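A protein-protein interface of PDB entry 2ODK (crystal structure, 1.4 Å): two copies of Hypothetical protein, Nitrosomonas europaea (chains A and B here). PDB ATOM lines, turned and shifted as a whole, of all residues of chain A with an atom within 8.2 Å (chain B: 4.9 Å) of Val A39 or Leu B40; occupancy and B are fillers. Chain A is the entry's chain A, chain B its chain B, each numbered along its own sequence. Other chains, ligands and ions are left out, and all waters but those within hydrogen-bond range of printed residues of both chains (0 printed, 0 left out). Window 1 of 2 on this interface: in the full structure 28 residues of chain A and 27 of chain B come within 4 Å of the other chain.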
ATOM      1  N   MET A   3      25.712  -8.620   2.715  1.00  0.00           N
ATOM      2  CA  MET A   3      26.768  -7.706   3.240  1.00  0.00           C
ATOM      3  C   MET A   3      28.159  -8.346   3.069  1.00  0.00           C
ATOM      4  O   MET A   3      29.089  -7.997   3.794  1.00  0.00           O
ATOM      5  CB  MET A   3      26.518  -7.319   4.711  1.00  0.00           C
ATOM      6  CG  MET A   3      25.266  -6.448   4.984  1.00  0.00           C
ATOM      7  SD  MET A   3      25.241  -4.675   4.162  1.00  0.00           S
ATOM      8  CE  MET A   3      23.715  -3.939   5.151  1.00  0.00           C
ATOM      9  N   HIS A   4      28.290  -9.289   2.133  1.00  0.00           N
ATOM     10  CA  HIS A   4      29.605  -9.619   1.561  1.00  0.00           C
ATOM     11  C   HIS A   4      30.228  -8.308   1.085  1.00  0.00           C
ATOM     12  O   HIS A   4      29.484  -7.360   0.703  1.00  0.00           O
ATOM     13  CB  HIS A   4      29.460 -10.575   0.379  1.00  0.00           C
ATOM     14  CG  HIS A   4      30.761 -10.963  -0.265  1.00  0.00           C
ATOM     15  ND1 HIS A   4      31.718 -11.730   0.374  1.00  0.00           N
ATOM     16  CD2 HIS A   4      31.271 -10.676  -1.490  1.00  0.00           C
ATOM     17  CE1 HIS A   4      32.759 -11.892  -0.428  1.00  0.00           C
ATOM     18  NE2 HIS A   4      32.512 -11.266  -1.566  1.00  0.00           N
ATOM     19  N   VAL A   8      36.593  -2.713  -5.068  1.00  0.00           N
ATOM     20  CA  VAL A   8      36.116  -2.010  -6.271  1.00  0.00           C
ATOM     21  C   VAL A   8      36.414  -2.760  -7.577  1.00  0.00           C
ATOM     22  O   VAL A   8      35.538  -2.890  -8.453  1.00  0.00           O
ATOM     23  CB  VAL A   8      36.583  -0.521  -6.271  1.00  0.00           C
ATOM     24  CG1 VAL A   8      38.111  -0.425  -6.310  1.00  0.00           C
ATOM     25  CG2 VAL A   8      35.919   0.228  -7.436  1.00  0.00           C
ATOM     26  N   ALA A  11      34.086  -5.903  -7.823  1.00  0.00           N
ATOM     27  CA  ALA A  11      32.702  -5.565  -8.151  1.00  0.00           C
ATOM     28  C   ALA A  11      32.612  -5.178  -9.634  1.00  0.00           C
ATOM     29  O   ALA A  11      31.578  -5.445 -10.285  1.00  0.00           O
ATOM     30  CB  ALA A  11      32.220  -4.408  -7.251  1.00  0.00           C
ATOM     31  N   PHE A  15      30.686  -7.628 -12.167  1.00  0.00           N
ATOM     32  CA  PHE A  15      29.509  -6.784 -11.930  1.00  0.00           C
ATOM     33  C   PHE A  15      28.190  -7.558 -11.980  1.00  0.00           C
ATOM     34  O   PHE A  15      27.295  -7.352 -11.125  1.00  0.00           O
ATOM     35  CB  PHE A  15      29.459  -5.593 -12.885  1.00  0.00           C
ATOM     36  CG  PHE A  15      28.399  -4.599 -12.512  1.00  0.00           C
ATOM     37  CD1 PHE A  15      28.610  -3.707 -11.489  1.00  0.00           C
ATOM     38  CD2 PHE A  15      27.147  -4.607 -13.155  1.00  0.00           C
ATOM     39  CE1 PHE A  15      27.625  -2.790 -11.108  1.00  0.00           C
ATOM     40  CE2 PHE A  15      26.153  -3.673 -12.743  1.00  0.00           C
ATOM     41  CZ  PHE A  15      26.397  -2.798 -11.740  1.00  0.00           C
ATOM     42  N   PHE A  18      27.828  -9.446  -8.803  1.00  0.00           N
ATOM     43  CA  PHE A  18      27.642  -8.478  -7.717  1.00  0.00           C
ATOM     44  C   PHE A  18      26.169  -8.021  -7.677  1.00  0.00           C
ATOM     45  O   PHE A  18      25.543  -8.012  -6.604  1.00  0.00           O
ATOM     46  CB  PHE A  18      28.614  -7.320  -8.024  1.00  0.00           C
ATOM     47  CG  PHE A  18      28.494  -6.095  -7.151  1.00  0.00           C
ATOM     48  CD1 PHE A  18      28.754  -6.133  -5.785  1.00  0.00           C
ATOM     49  CD2 PHE A  18      28.214  -4.845  -7.729  1.00  0.00           C
ATOM     50  CE1 PHE A  18      28.724  -4.967  -5.002  1.00  0.00           C
ATOM     51  CE2 PHE A  18      28.181  -3.705  -6.965  1.00  0.00           C
ATOM     52  CZ  PHE A  18      28.430  -3.734  -5.621  1.00  0.00           C
ATOM     53  N   CYS A  22      23.166  -8.907  -4.921  1.00  0.00           N
ATOM     54  CA  CYS A  22      22.313  -7.864  -4.293  1.00  0.00           C
ATOM     55  C   CYS A  22      20.842  -8.324  -4.299  1.00  0.00           C
ATOM     56  O   CYS A  22      20.128  -8.248  -3.285  1.00  0.00           O
ATOM     57  CB  CYS A  22      22.507  -6.578  -5.074  1.00  0.00           C
ATOM     58  SG  CYS A  22      21.369  -5.270  -4.640  1.00  0.00           S
ATOM     59  N   GLY A  26      20.868  -9.797  -0.828  1.00  0.00           N
ATOM     60  CA  GLY A  26      20.701  -8.579  -0.065  1.00  0.00           C
ATOM     61  C   GLY A  26      21.875  -7.623  -0.277  1.00  0.00           C
ATOM     62  O   GLY A  26      22.763  -7.882  -1.082  1.00  0.00           O
ATOM     63  N   PRO A  27      21.822  -6.499   0.412  1.00  0.00           N
ATOM     64  CA  PRO A  27      22.860  -5.450   0.246  1.00  0.00           C
ATOM     65  C   PRO A  27      24.279  -5.999   0.197  1.00  0.00           C
ATOM     66  O   PRO A  27      24.662  -6.821   1.047  1.00  0.00           O
ATOM     67  CB  PRO A  27      22.644  -4.569   1.465  1.00  0.00           C
ATOM     68  CG  PRO A  27      21.093  -4.650   1.659  1.00  0.00           C
ATOM     69  CD  PRO A  27      20.780  -6.099   1.381  1.00  0.00           C
ATOM     70  N   GLN A  28      25.037  -5.543  -0.795  1.00  0.00           N
ATOM     71  CA  GLN A  28      26.435  -5.964  -0.989  1.00  0.00           C
ATOM     72  C   GLN A  28      27.327  -4.745  -0.786  1.00  0.00           C
ATOM     73  O   GLN A  28      27.056  -3.703  -1.384  1.00  0.00           O
ATOM     74  CB  GLN A  28      26.633  -6.498  -2.422  1.00  0.00           C
ATOM     75  CG  GLN A  28      25.734  -7.696  -2.781  1.00  0.00           C
ATOM     76  CD  GLN A  28      26.109  -8.924  -1.978  1.00  0.00           C
ATOM     77  OE1 GLN A  28      27.263  -9.375  -2.012  1.00  0.00           O
ATOM     78  NE2 GLN A  28      25.127  -9.489  -1.244  1.00  0.00           N
ATOM     79  N   ILE A  29      28.340  -4.848   0.074  1.00  0.00           N
ATOM     80  CA  ILE A  29      29.242  -3.716   0.321  1.00  0.00           C
ATOM     81  C   ILE A  29      30.354  -3.656  -0.715  1.00  0.00           C
ATOM     82  O   ILE A  29      30.821  -4.691  -1.181  1.00  0.00           O
ATOM     83  CB  ILE A  29      29.834  -3.854   1.721  1.00  0.00           C
ATOM     84  CG1 ILE A  29      28.684  -3.742   2.741  1.00  0.00           C
ATOM     85  CG2 ILE A  29      30.897  -2.752   1.956  1.00  0.00           C
ATOM     86  CD1 ILE A  29      29.034  -4.058   4.217  1.00  0.00           C
ATOM     87  N   VAL A  30      30.737  -2.439  -1.087  1.00  0.00           N
ATOM     88  CA  VAL A  30      31.890  -2.220  -1.949  1.00  0.00           C
ATOM     89  C   VAL A  30      32.972  -1.515  -1.134  1.00  0.00           C
ATOM     90  O   VAL A  30      32.667  -0.541  -0.438  1.00  0.00           O
ATOM     91  CB  VAL A  30      31.495  -1.288  -3.096  1.00  0.00           C
ATOM     92  CG1 VAL A  30      32.696  -1.005  -4.021  1.00  0.00           C
ATOM     93  CG2 VAL A  30      30.326  -1.897  -3.869  1.00  0.00           C
ATOM     94  N   SER A  31      34.223  -1.980  -1.240  1.00  0.00           N
ATOM     95  CA  SER A  31      35.333  -1.341  -0.544  1.00  0.00           C
ATOM     96  C   SER A  31      36.355  -0.741  -1.520  1.00  0.00           C
ATOM     97  O   SER A  31      36.425  -1.149  -2.707  1.00  0.00           O
ATOM     98  CB  SER A  31      36.029  -2.372   0.345  1.00  0.00           C
ATOM     99  OG  SER A  31      36.582  -3.429  -0.417  1.00  0.00           O
ATOM    100  N   GLU A  36      35.266  -0.142   3.836  1.00  0.00           N
ATOM    101  CA  GLU A  36      33.900  -0.134   3.305  1.00  0.00           C
ATOM    102  C   GLU A  36      33.529   1.282   2.865  1.00  0.00           C
ATOM    103  O   GLU A  36      33.738   2.272   3.625  1.00  0.00           O
ATOM    104  CB  GLU A  36      32.944  -0.677   4.377  1.00  0.00           C
ATOM    105  CG  GLU A  36      33.267  -2.120   4.719  1.00  0.00           C
ATOM    106  CD  GLU A  36      32.315  -2.736   5.733  1.00  0.00           C
ATOM    107  OE1 GLU A  36      31.366  -2.060   6.142  1.00  0.00           O
ATOM    108  OE2 GLU A  36      32.533  -3.894   6.084  1.00  0.00           O
ATOM    109  N   GLU A  37      32.972   1.411   1.654  1.00  0.00           N
ATOM    110  CA  GLU A  37      32.700   2.733   1.088  1.00  0.00           C
ATOM    111  C   GLU A  37      31.217   2.917   0.744  1.00  0.00           C
ATOM    112  O   GLU A  37      30.682   4.029   0.892  1.00  0.00           O
ATOM    113  CB  GLU A  37      33.559   2.991  -0.164  1.00  0.00           C
ATOM    114  CG  GLU A  37      35.047   3.269   0.193  1.00  0.00           C
ATOM    115  CD  GLU A  37      35.240   4.599   0.918  1.00  0.00           C
ATOM    116  OE1 GLU A  37      34.264   5.381   0.960  1.00  0.00           O
ATOM    117  OE2 GLU A  37      36.336   4.872   1.460  1.00  0.00           O
ATOM    118  N   ALA A  38      30.602   1.865   0.210  1.00  0.00           N
ATOM    119  CA  ALA A  38      29.233   2.008  -0.290  1.00  0.00           C
ATOM    120  C   ALA A  38      28.533   0.683  -0.277  1.00  0.00           C
ATOM    121  O   ALA A  38      29.158  -0.339  -0.029  1.00  0.00           O
ATOM    122  CB  ALA A  38      29.242   2.616  -1.706  1.00  0.00           C
ATOM    123  N   VAL A  39      27.219   0.682  -0.522  1.00  0.00           N
ATOM    124  CA  VAL A  39      26.484  -0.583  -0.460  1.00  0.00           C
ATOM    125  C   VAL A  39      25.460  -0.592  -1.597  1.00  0.00           C
ATOM    126  O   VAL A  39      24.808   0.421  -1.872  1.00  0.00           O
ATOM    127  CB  VAL A  39      25.868  -0.792   0.946  1.00  0.00           C
ATOM    128  CG1 VAL A  39      25.040   0.379   1.354  1.00  0.00           C
ATOM    129  CG2 VAL A  39      25.061  -2.064   1.029  1.00  0.00           C
ATOM    130  N   LEU A  40      25.419  -1.717  -2.311  1.00  0.00           N
ATOM    131  CA  LEU A  40      24.445  -1.849  -3.415  1.00  0.00           C
ATOM    132  C   LEU A  40      23.210  -2.502  -2.818  1.00  0.00           C
ATOM    133  O   LEU A  40      23.307  -3.626  -2.291  1.00  0.00           O
ATOM    134  CB  LEU A  40      25.022  -2.739  -4.531  1.00  0.00           C
ATOM    135  CG  LEU A  40      24.200  -2.731  -5.826  1.00  0.00           C
ATOM    136  CD1 LEU A  40      24.262  -1.396  -6.556  1.00  0.00           C
ATOM    137  CD2 LEU A  40      24.568  -3.875  -6.756  1.00  0.00           C
ATOM    138  N   VAL A  41      22.073  -1.794  -2.900  1.00  0.00           N
ATOM    139  CA  VAL A  41      20.848  -2.185  -2.203  1.00  0.00           C
ATOM    140  C   VAL A  41      19.764  -2.451  -3.258  1.00  0.00           C
ATOM    141  O   VAL A  41      19.652  -1.710  -4.207  1.00  0.00           O
ATOM    142  CB  VAL A  41      20.363  -1.005  -1.308  1.00  0.00           C
ATOM    143  CG1 VAL A  41      19.048  -1.326  -0.594  1.00  0.00           C
ATOM    144  CG2 VAL A  41      21.475  -0.600  -0.307  1.00  0.00           C
ATOM    145  N   PRO A  42      18.949  -3.510  -3.078  1.00  0.00           N
ATOM    146  CA  PRO A  42      17.839  -3.696  -4.025  1.00  0.00           C
ATOM    147  C   PRO A  42      16.972  -2.442  -4.030  1.00  0.00           C
ATOM    148  O   PRO A  42      16.675  -1.891  -2.978  1.00  0.00           O
ATOM    149  CB  PRO A  42      17.037  -4.859  -3.419  1.00  0.00           C
ATOM    150  CG  PRO A  42      18.037  -5.617  -2.536  1.00  0.00           C
ATOM    151  CD  PRO A  42      18.980  -4.531  -2.011  1.00  0.00           C
ATOM    152  N   ILE A  43      16.540  -2.002  -5.205  1.00  0.00           N
ATOM    153  CA  ILE A  43      15.933  -0.675  -5.273  1.00  0.00           C
ATOM    154  C   ILE A  43      14.646  -0.594  -4.420  1.00  0.00           C
ATOM    155  O   ILE A  43      14.399   0.417  -3.737  1.00  0.00           O
ATOM    156  CB  ILE A  43      15.679  -0.227  -6.724  1.00  0.00           C
ATOM    157  CG1 ILE A  43      15.221   1.242  -6.826  1.00  0.00           C
ATOM    158  CG2 ILE A  43      14.685  -1.116  -7.453  1.00  0.00           C
ATOM    159  CD1 ILE A  43      16.373   2.211  -6.476  1.00  0.00           C
ATOM    160  N   GLU A  45      13.950  -2.158  -1.679  1.00  0.00           N
ATOM    161  CA  GLU A  45      14.298  -2.051  -0.269  1.00  0.00           C
ATOM    162  C   GLU A  45      14.692  -0.607   0.069  1.00  0.00           C
ATOM    163  O   GLU A  45      14.274  -0.069   1.112  1.00  0.00           O
ATOM    164  CB  GLU A  45      15.460  -2.999   0.043  1.00  0.00           C
ATOM    165  CG  GLU A  45      15.948  -2.913   1.474  1.00  0.00           C
ATOM    166  CD  GLU A  45      16.960  -4.003   1.833  1.00  0.00           C
ATOM    167  OE1 GLU A  45      16.993  -5.043   1.147  1.00  0.00           O
ATOM    168  OE2 GLU A  45      17.714  -3.830   2.829  1.00  0.00           O
ATOM    169  N   TRP A  46      15.494   0.028  -0.815  1.00  0.00           N
ATOM    170  CA  TRP A  46      15.834   1.418  -0.625  1.00  0.00           C
ATOM    171  C   TRP A  46      14.592   2.324  -0.596  1.00  0.00           C
ATOM    172  O   TRP A  46      14.461   3.198   0.294  1.00  0.00           O
ATOM    173  CB  TRP A  46      16.761   1.827  -1.783  1.00  0.00           C
ATOM    174  CG  TRP A  46      17.035   3.294  -1.932  1.00  0.00           C
ATOM    175  CD1 TRP A  46      16.603   4.145  -2.945  1.00  0.00           C
ATOM    176  CD2 TRP A  46      17.819   4.049  -1.072  1.00  0.00           C
ATOM    177  NE1 TRP A  46      17.095   5.399  -2.726  1.00  0.00           N
ATOM    178  CE2 TRP A  46      17.863   5.375  -1.592  1.00  0.00           C
ATOM    179  CE3 TRP A  46      18.534   3.747   0.059  1.00  0.00           C
ATOM    180  CZ2 TRP A  46      18.559   6.392  -0.982  1.00  0.00           C
ATOM    181  CZ3 TRP A  46      19.257   4.808   0.687  1.00  0.00           C
ATOM    182  CH2 TRP A  46      19.258   6.085   0.157  1.00  0.00           C
ATOM    183  N   PHE B  18      31.063   5.453 -11.266  1.00  0.00           N
ATOM    184  CA  PHE B  18      29.768   5.170 -10.592  1.00  0.00           C
ATOM    185  C   PHE B  18      29.957   5.226  -9.056  1.00  0.00           C
ATOM    186  O   PHE B  18      29.177   5.884  -8.345  1.00  0.00           O
ATOM    187  CB  PHE B  18      29.338   3.790 -11.090  1.00  0.00           C
ATOM    188  CG  PHE B  18      28.099   3.183 -10.447  1.00  0.00           C
ATOM    189  CD1 PHE B  18      26.843   3.713 -10.653  1.00  0.00           C
ATOM    190  CD2 PHE B  18      28.221   1.967  -9.799  1.00  0.00           C
ATOM    191  CE1 PHE B  18      25.696   3.061 -10.104  1.00  0.00           C
ATOM    192  CE2 PHE B  18      27.097   1.320  -9.271  1.00  0.00           C
ATOM    193  CZ  PHE B  18      25.862   1.878  -9.419  1.00  0.00           C
ATOM    194  N   LEU B  19      31.035   4.609  -8.548  1.00  0.00           N
ATOM    195  CA  LEU B  19      31.287   4.645  -7.088  1.00  0.00           C
ATOM    196  C   LEU B  19      31.688   6.046  -6.641  1.00  0.00           C
ATOM    197  O   LEU B  19      31.220   6.537  -5.605  1.00  0.00           O
ATOM    198  CB  LEU B  19      32.364   3.599  -6.756  1.00  0.00           C
ATOM    199  CG  LEU B  19      32.831   3.569  -5.308  1.00  0.00           C
ATOM    200  CD1 LEU B  19      31.668   3.305  -4.334  1.00  0.00           C
ATOM    201  CD2 LEU B  19      33.865   2.469  -5.119  1.00  0.00           C
ATOM    202  N   CYS B  22      28.594   8.099  -6.454  1.00  0.00           N
ATOM    203  CA  CYS B  22      27.824   7.750  -5.240  1.00  0.00           C
ATOM    204  C   CYS B  22      28.308   8.558  -4.024  1.00  0.00           C
ATOM    205  O   CYS B  22      27.538   9.167  -3.281  1.00  0.00           O
ATOM    206  CB  CYS B  22      27.985   6.240  -5.040  1.00  0.00           C
ATOM    207  SG  CYS B  22      27.560   5.641  -3.410  1.00  0.00           S
ATOM    208  N   GLY B  26      25.754  11.389  -4.305  1.00  0.00           N
ATOM    209  CA  GLY B  26      24.633  10.702  -3.641  1.00  0.00           C
ATOM    210  C   GLY B  26      24.265   9.419  -4.364  1.00  0.00           C
ATOM    211  O   GLY B  26      24.861   9.042  -5.369  1.00  0.00           O
ATOM    212  N   PRO B  27      23.256   8.715  -3.856  1.00  0.00           N
ATOM    213  CA  PRO B  27      22.860   7.402  -4.389  1.00  0.00           C
ATOM    214  C   PRO B  27      22.764   7.385  -5.906  1.00  0.00           C
ATOM    215  O   PRO B  27      22.172   8.312  -6.516  1.00  0.00           O
ATOM    216  CB  PRO B  27      21.496   7.155  -3.716  1.00  0.00           C
ATOM    217  CG  PRO B  27      21.623   7.889  -2.354  1.00  0.00           C
ATOM    218  CD  PRO B  27      22.456   9.142  -2.692  1.00  0.00           C
ATOM    219  N   GLN B  28      23.301   6.318  -6.509  1.00  0.00           N
ATOM    220  CA  GLN B  28      23.303   6.152  -7.970  1.00  0.00           C
ATOM    221  C   GLN B  28      22.508   4.878  -8.288  1.00  0.00           C
ATOM    222  O   GLN B  28      22.826   3.817  -7.747  1.00  0.00           O
ATOM    223  CB  GLN B  28      24.756   5.990  -8.475  1.00  0.00           C
ATOM    224  CG  GLN B  28      25.647   7.188  -8.106  1.00  0.00           C
ATOM    225  CD  GLN B  28      25.251   8.482  -8.809  1.00  0.00           C
ATOM    226  OE1 GLN B  28      25.047   9.539  -8.155  1.00  0.00           O
ATOM    227  NE2 GLN B  28      25.151   8.426 -10.105  1.00  0.00           N
ATOM    228  N   ALA B  38      18.667  -1.615  -8.695  1.00  0.00           N
ATOM    229  CA  ALA B  38      19.427  -1.502  -7.441  1.00  0.00           C
ATOM    230  C   ALA B  38      19.953  -0.085  -7.308  1.00  0.00           C
ATOM    231  O   ALA B  38      19.846   0.703  -8.267  1.00  0.00           O
ATOM    232  CB  ALA B  38      20.619  -2.523  -7.375  1.00  0.00           C
ATOM    233  N   VAL B  39      20.533   0.243  -6.156  1.00  0.00           N
ATOM    234  CA  VAL B  39      21.035   1.608  -5.960  1.00  0.00           C
ATOM    235  C   VAL B  39      22.292   1.494  -5.125  1.00  0.00           C
ATOM    236  O   VAL B  39      22.328   0.733  -4.147  1.00  0.00           O
ATOM    237  CB  VAL B  39      19.966   2.538  -5.298  1.00  0.00           C
ATOM    238  CG1 VAL B  39      19.375   1.918  -4.003  1.00  0.00           C
ATOM    239  CG2 VAL B  39      20.486   3.942  -5.088  1.00  0.00           C
ATOM    240  N   LEU B  40      23.335   2.242  -5.512  1.00  0.00           N
ATOM    241  CA  LEU B  40      24.580   2.255  -4.748  1.00  0.00           C
ATOM    242  C   LEU B  40      24.520   3.461  -3.819  1.00  0.00           C
ATOM    243  O   LEU B  40      24.400   4.593  -4.277  1.00  0.00           O
ATOM    244  CB  LEU B  40      25.744   2.382  -5.727  1.00  0.00           C
ATOM    245  CG  LEU B  40      27.115   2.136  -5.088  1.00  0.00           C
ATOM    246  CD1 LEU B  40      27.293   0.698  -4.607  1.00  0.00           C
ATOM    247  CD2 LEU B  40      28.235   2.545  -6.087  1.00  0.00           C
ATOM    248  N   VAL B  41      24.599   3.197  -2.509  1.00  0.00           N
ATOM    249  CA  VAL B  41      24.383   4.209  -1.477  1.00  0.00           C
ATOM    250  C   VAL B  41      25.681   4.345  -0.669  1.00  0.00           C
ATOM    251  O   VAL B  41      26.282   3.338  -0.281  1.00  0.00           O
ATOM    252  CB  VAL B  41      23.245   3.736  -0.506  1.00  0.00           C
ATOM    253  CG1 VAL B  41      22.960   4.775   0.584  1.00  0.00           C
ATOM    254  CG2 VAL B  41      21.958   3.394  -1.278  1.00  0.00           C
ATOM    255  N   PRO B  42      26.085   5.590  -0.377  1.00  0.00           N
ATOM    256  CA  PRO B  42      27.303   5.724   0.454  1.00  0.00           C
ATOM    257  C   PRO B  42      27.082   5.025   1.784  1.00  0.00           C
ATOM    258  O   PRO B  42      25.973   5.087   2.324  1.00  0.00           O
ATOM    259  CB  PRO B  42      27.432   7.230   0.673  1.00  0.00           C
ATOM    260  CG  PRO B  42      26.571   7.860  -0.387  1.00  0.00           C
ATOM    261  CD  PRO B  42      25.484   6.883  -0.767  1.00  0.00           C
ATOM    262  N   ILE B  43      28.103   4.376   2.337  1.00  0.00           N
ATOM    263  CA  ILE B  43      27.918   3.494   3.488  1.00  0.00           C
ATOM    264  C   ILE B  43      27.368   4.226   4.731  1.00  0.00           C
ATOM    265  O   ILE B  43      26.519   3.690   5.469  1.00  0.00           O
ATOM    266  CB  ILE B  43      29.226   2.739   3.792  1.00  0.00           C
ATOM    267  CG1 ILE B  43      28.975   1.616   4.800  1.00  0.00           C
ATOM    268  CG2 ILE B  43      30.350   3.729   4.212  1.00  0.00           C
ATOM    269  CD1 ILE B  43      28.009   0.524   4.293  1.00  0.00           C
ATOM    270  N   TRP B  46      23.688   4.933   4.230  1.00  0.00           N
ATOM    271  CA  TRP B  46      22.938   3.687   4.431  1.00  0.00           C
ATOM    272  C   TRP B  46      22.694   3.410   5.916  1.00  0.00           C
ATOM    273  O   TRP B  46      21.547   3.136   6.343  1.00  0.00           O
ATOM    274  CB  TRP B  46      23.704   2.529   3.809  1.00  0.00           C
ATOM    275  CG  TRP B  46      23.121   1.187   4.049  1.00  0.00           C
ATOM    276  CD1 TRP B  46      23.707   0.133   4.715  1.00  0.00           C
ATOM    277  CD2 TRP B  46      21.859   0.716   3.573  1.00  0.00           C
ATOM    278  NE1 TRP B  46      22.867  -0.955   4.693  1.00  0.00           N
ATOM    279  CE2 TRP B  46      21.725  -0.627   4.016  1.00  0.00           C
ATOM    280  CE3 TRP B  46      20.809   1.303   2.856  1.00  0.00           C
ATOM    281  CZ2 TRP B  46      20.595  -1.403   3.743  1.00  0.00           C
ATOM    282  CZ3 TRP B  46      19.661   0.509   2.585  1.00  0.00           C
ATOM    283  CH2 TRP B  46      19.587  -0.824   3.025  1.00  0.00           C
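Phe A15 touches none of the printed residues of chain B. Printed residues of chain B within 4 Å of Pro A27: Trp B46 (3.9 Å). Of the printed residues of chain B, Val A39 touches Val B39 (3.4 Å), Leu B40 (3.4 Å), Val B41 (2.8 Å) and Trp B46 (3.4 Å). Of the printed residues of chain B, Leu A40 touches Ala B38 (3.9 Å), Val B39 (3.4 Å) and Leu B40 (3.8 Å). Printed residues of chain B within 4 Å of Glu A45: Trp B46. Of the printed residues of chain A, Leu B40 touches Ala A38, Val A39 and Leu A40. Printed residues of chain A within 4 Å of Pro B42: Glu A37. The nearest printed residue of chain A that does not touch Leu B40 is Val A30 (4.1 Å). The nearest printed residue of chain B that does not touch Met A3 is Ile B43 (5.9 Å).
The backbone carbonyl oxygen (O) of Pro A27 is in hydrogen-bond range of the backbone NH (N) of Met A3, at 2.7 Å. N of Val A8 is in hydrogen-bond range of O of Ser A31, at 2.8 Å. The backbone carbonyl oxygen (O) of Gln A28 is in hydrogen-bond range of the backbone NH (N) of Leu A40 (2.7 Å). N of Glu A37 lies within hydrogen-bond range of O of Val A30. N of Val A30 is in hydrogen-bond range of O of Ala A38, 2.8 Å away. O of Leu B40 sits at hydrogen-bond distance from SG of Cys B22 (3.4 Å).
The backbone carbonyl oxygen of Glu A37 sits at hydrogen-bond distance from the backbone NH of Ile B43, 3.0 Å away. The backbone carbonyl oxygen of Val B41 sits at hydrogen-bond distance from the backbone NH of Val A39 (2.8 Å). N of Val A41 sits at hydrogen-bond distance from O of Val B39 (2.8 Å). O of Val B39 lies close to O of Val A39.
Pro A27 touches Trp B46, and with the chains exchanged Trp A46 touches Pro B27. Ala A38 touches Ile B43, and with the chains exchanged Ile A43 touches Ala B38. Val A41 touches Trp B46, and with the chains exchanged Trp A46 touches Val B41. Ile A43 touches Val B39, but with the chains exchanged Val A39 does not touch Ile B43 (4.2 Å). Positions printed for both chains: 18, 22, 26, 27, 28, 38, 39, 40, 41, 42, 43 and 46.
Among the printed residues, merely in contact across the chains: Met A3 with Trp B46, Val A8 with Leu B19, Cys A22 with Ala B38, Pro A27 with Trp B46, Val A30 with Leu B19, Glu A36 with Ile B43, Glu A37 with Pro B42, Ala A38 with Leu B19, Ala A38 with Cys B22, Ala A38 with Leu B40, Ala A38 with Val B41, Ala A38 with Ile B43, Val A39 with Leu B40, Val A39 with Trp B46, Leu A40 with Ala B38, Leu A40 with Val B39, Leu A40 with Leu B40, Val A41 with Ala B38, Val A41 with Trp B46, Ile A43 with Ala B38, Ile A43 with Val B39, Glu A45 with Trp B46, Trp A46 with Pro B27, Trp A46 with Val B39 and Trp A46 with Val B41.
Hydrophobic or aromatic side chains of chain A that line the printed part of chain B: Met A3, Val A8, Pro A27, Val A30, Ala A38, Val A39, Leu A40, Val A41, Ile A43 and Trp A46. Among the printed residues, no Asp or Glu carboxylate lies within 4 Å of a Lys or Arg side-chain nitrogen of the other chain.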
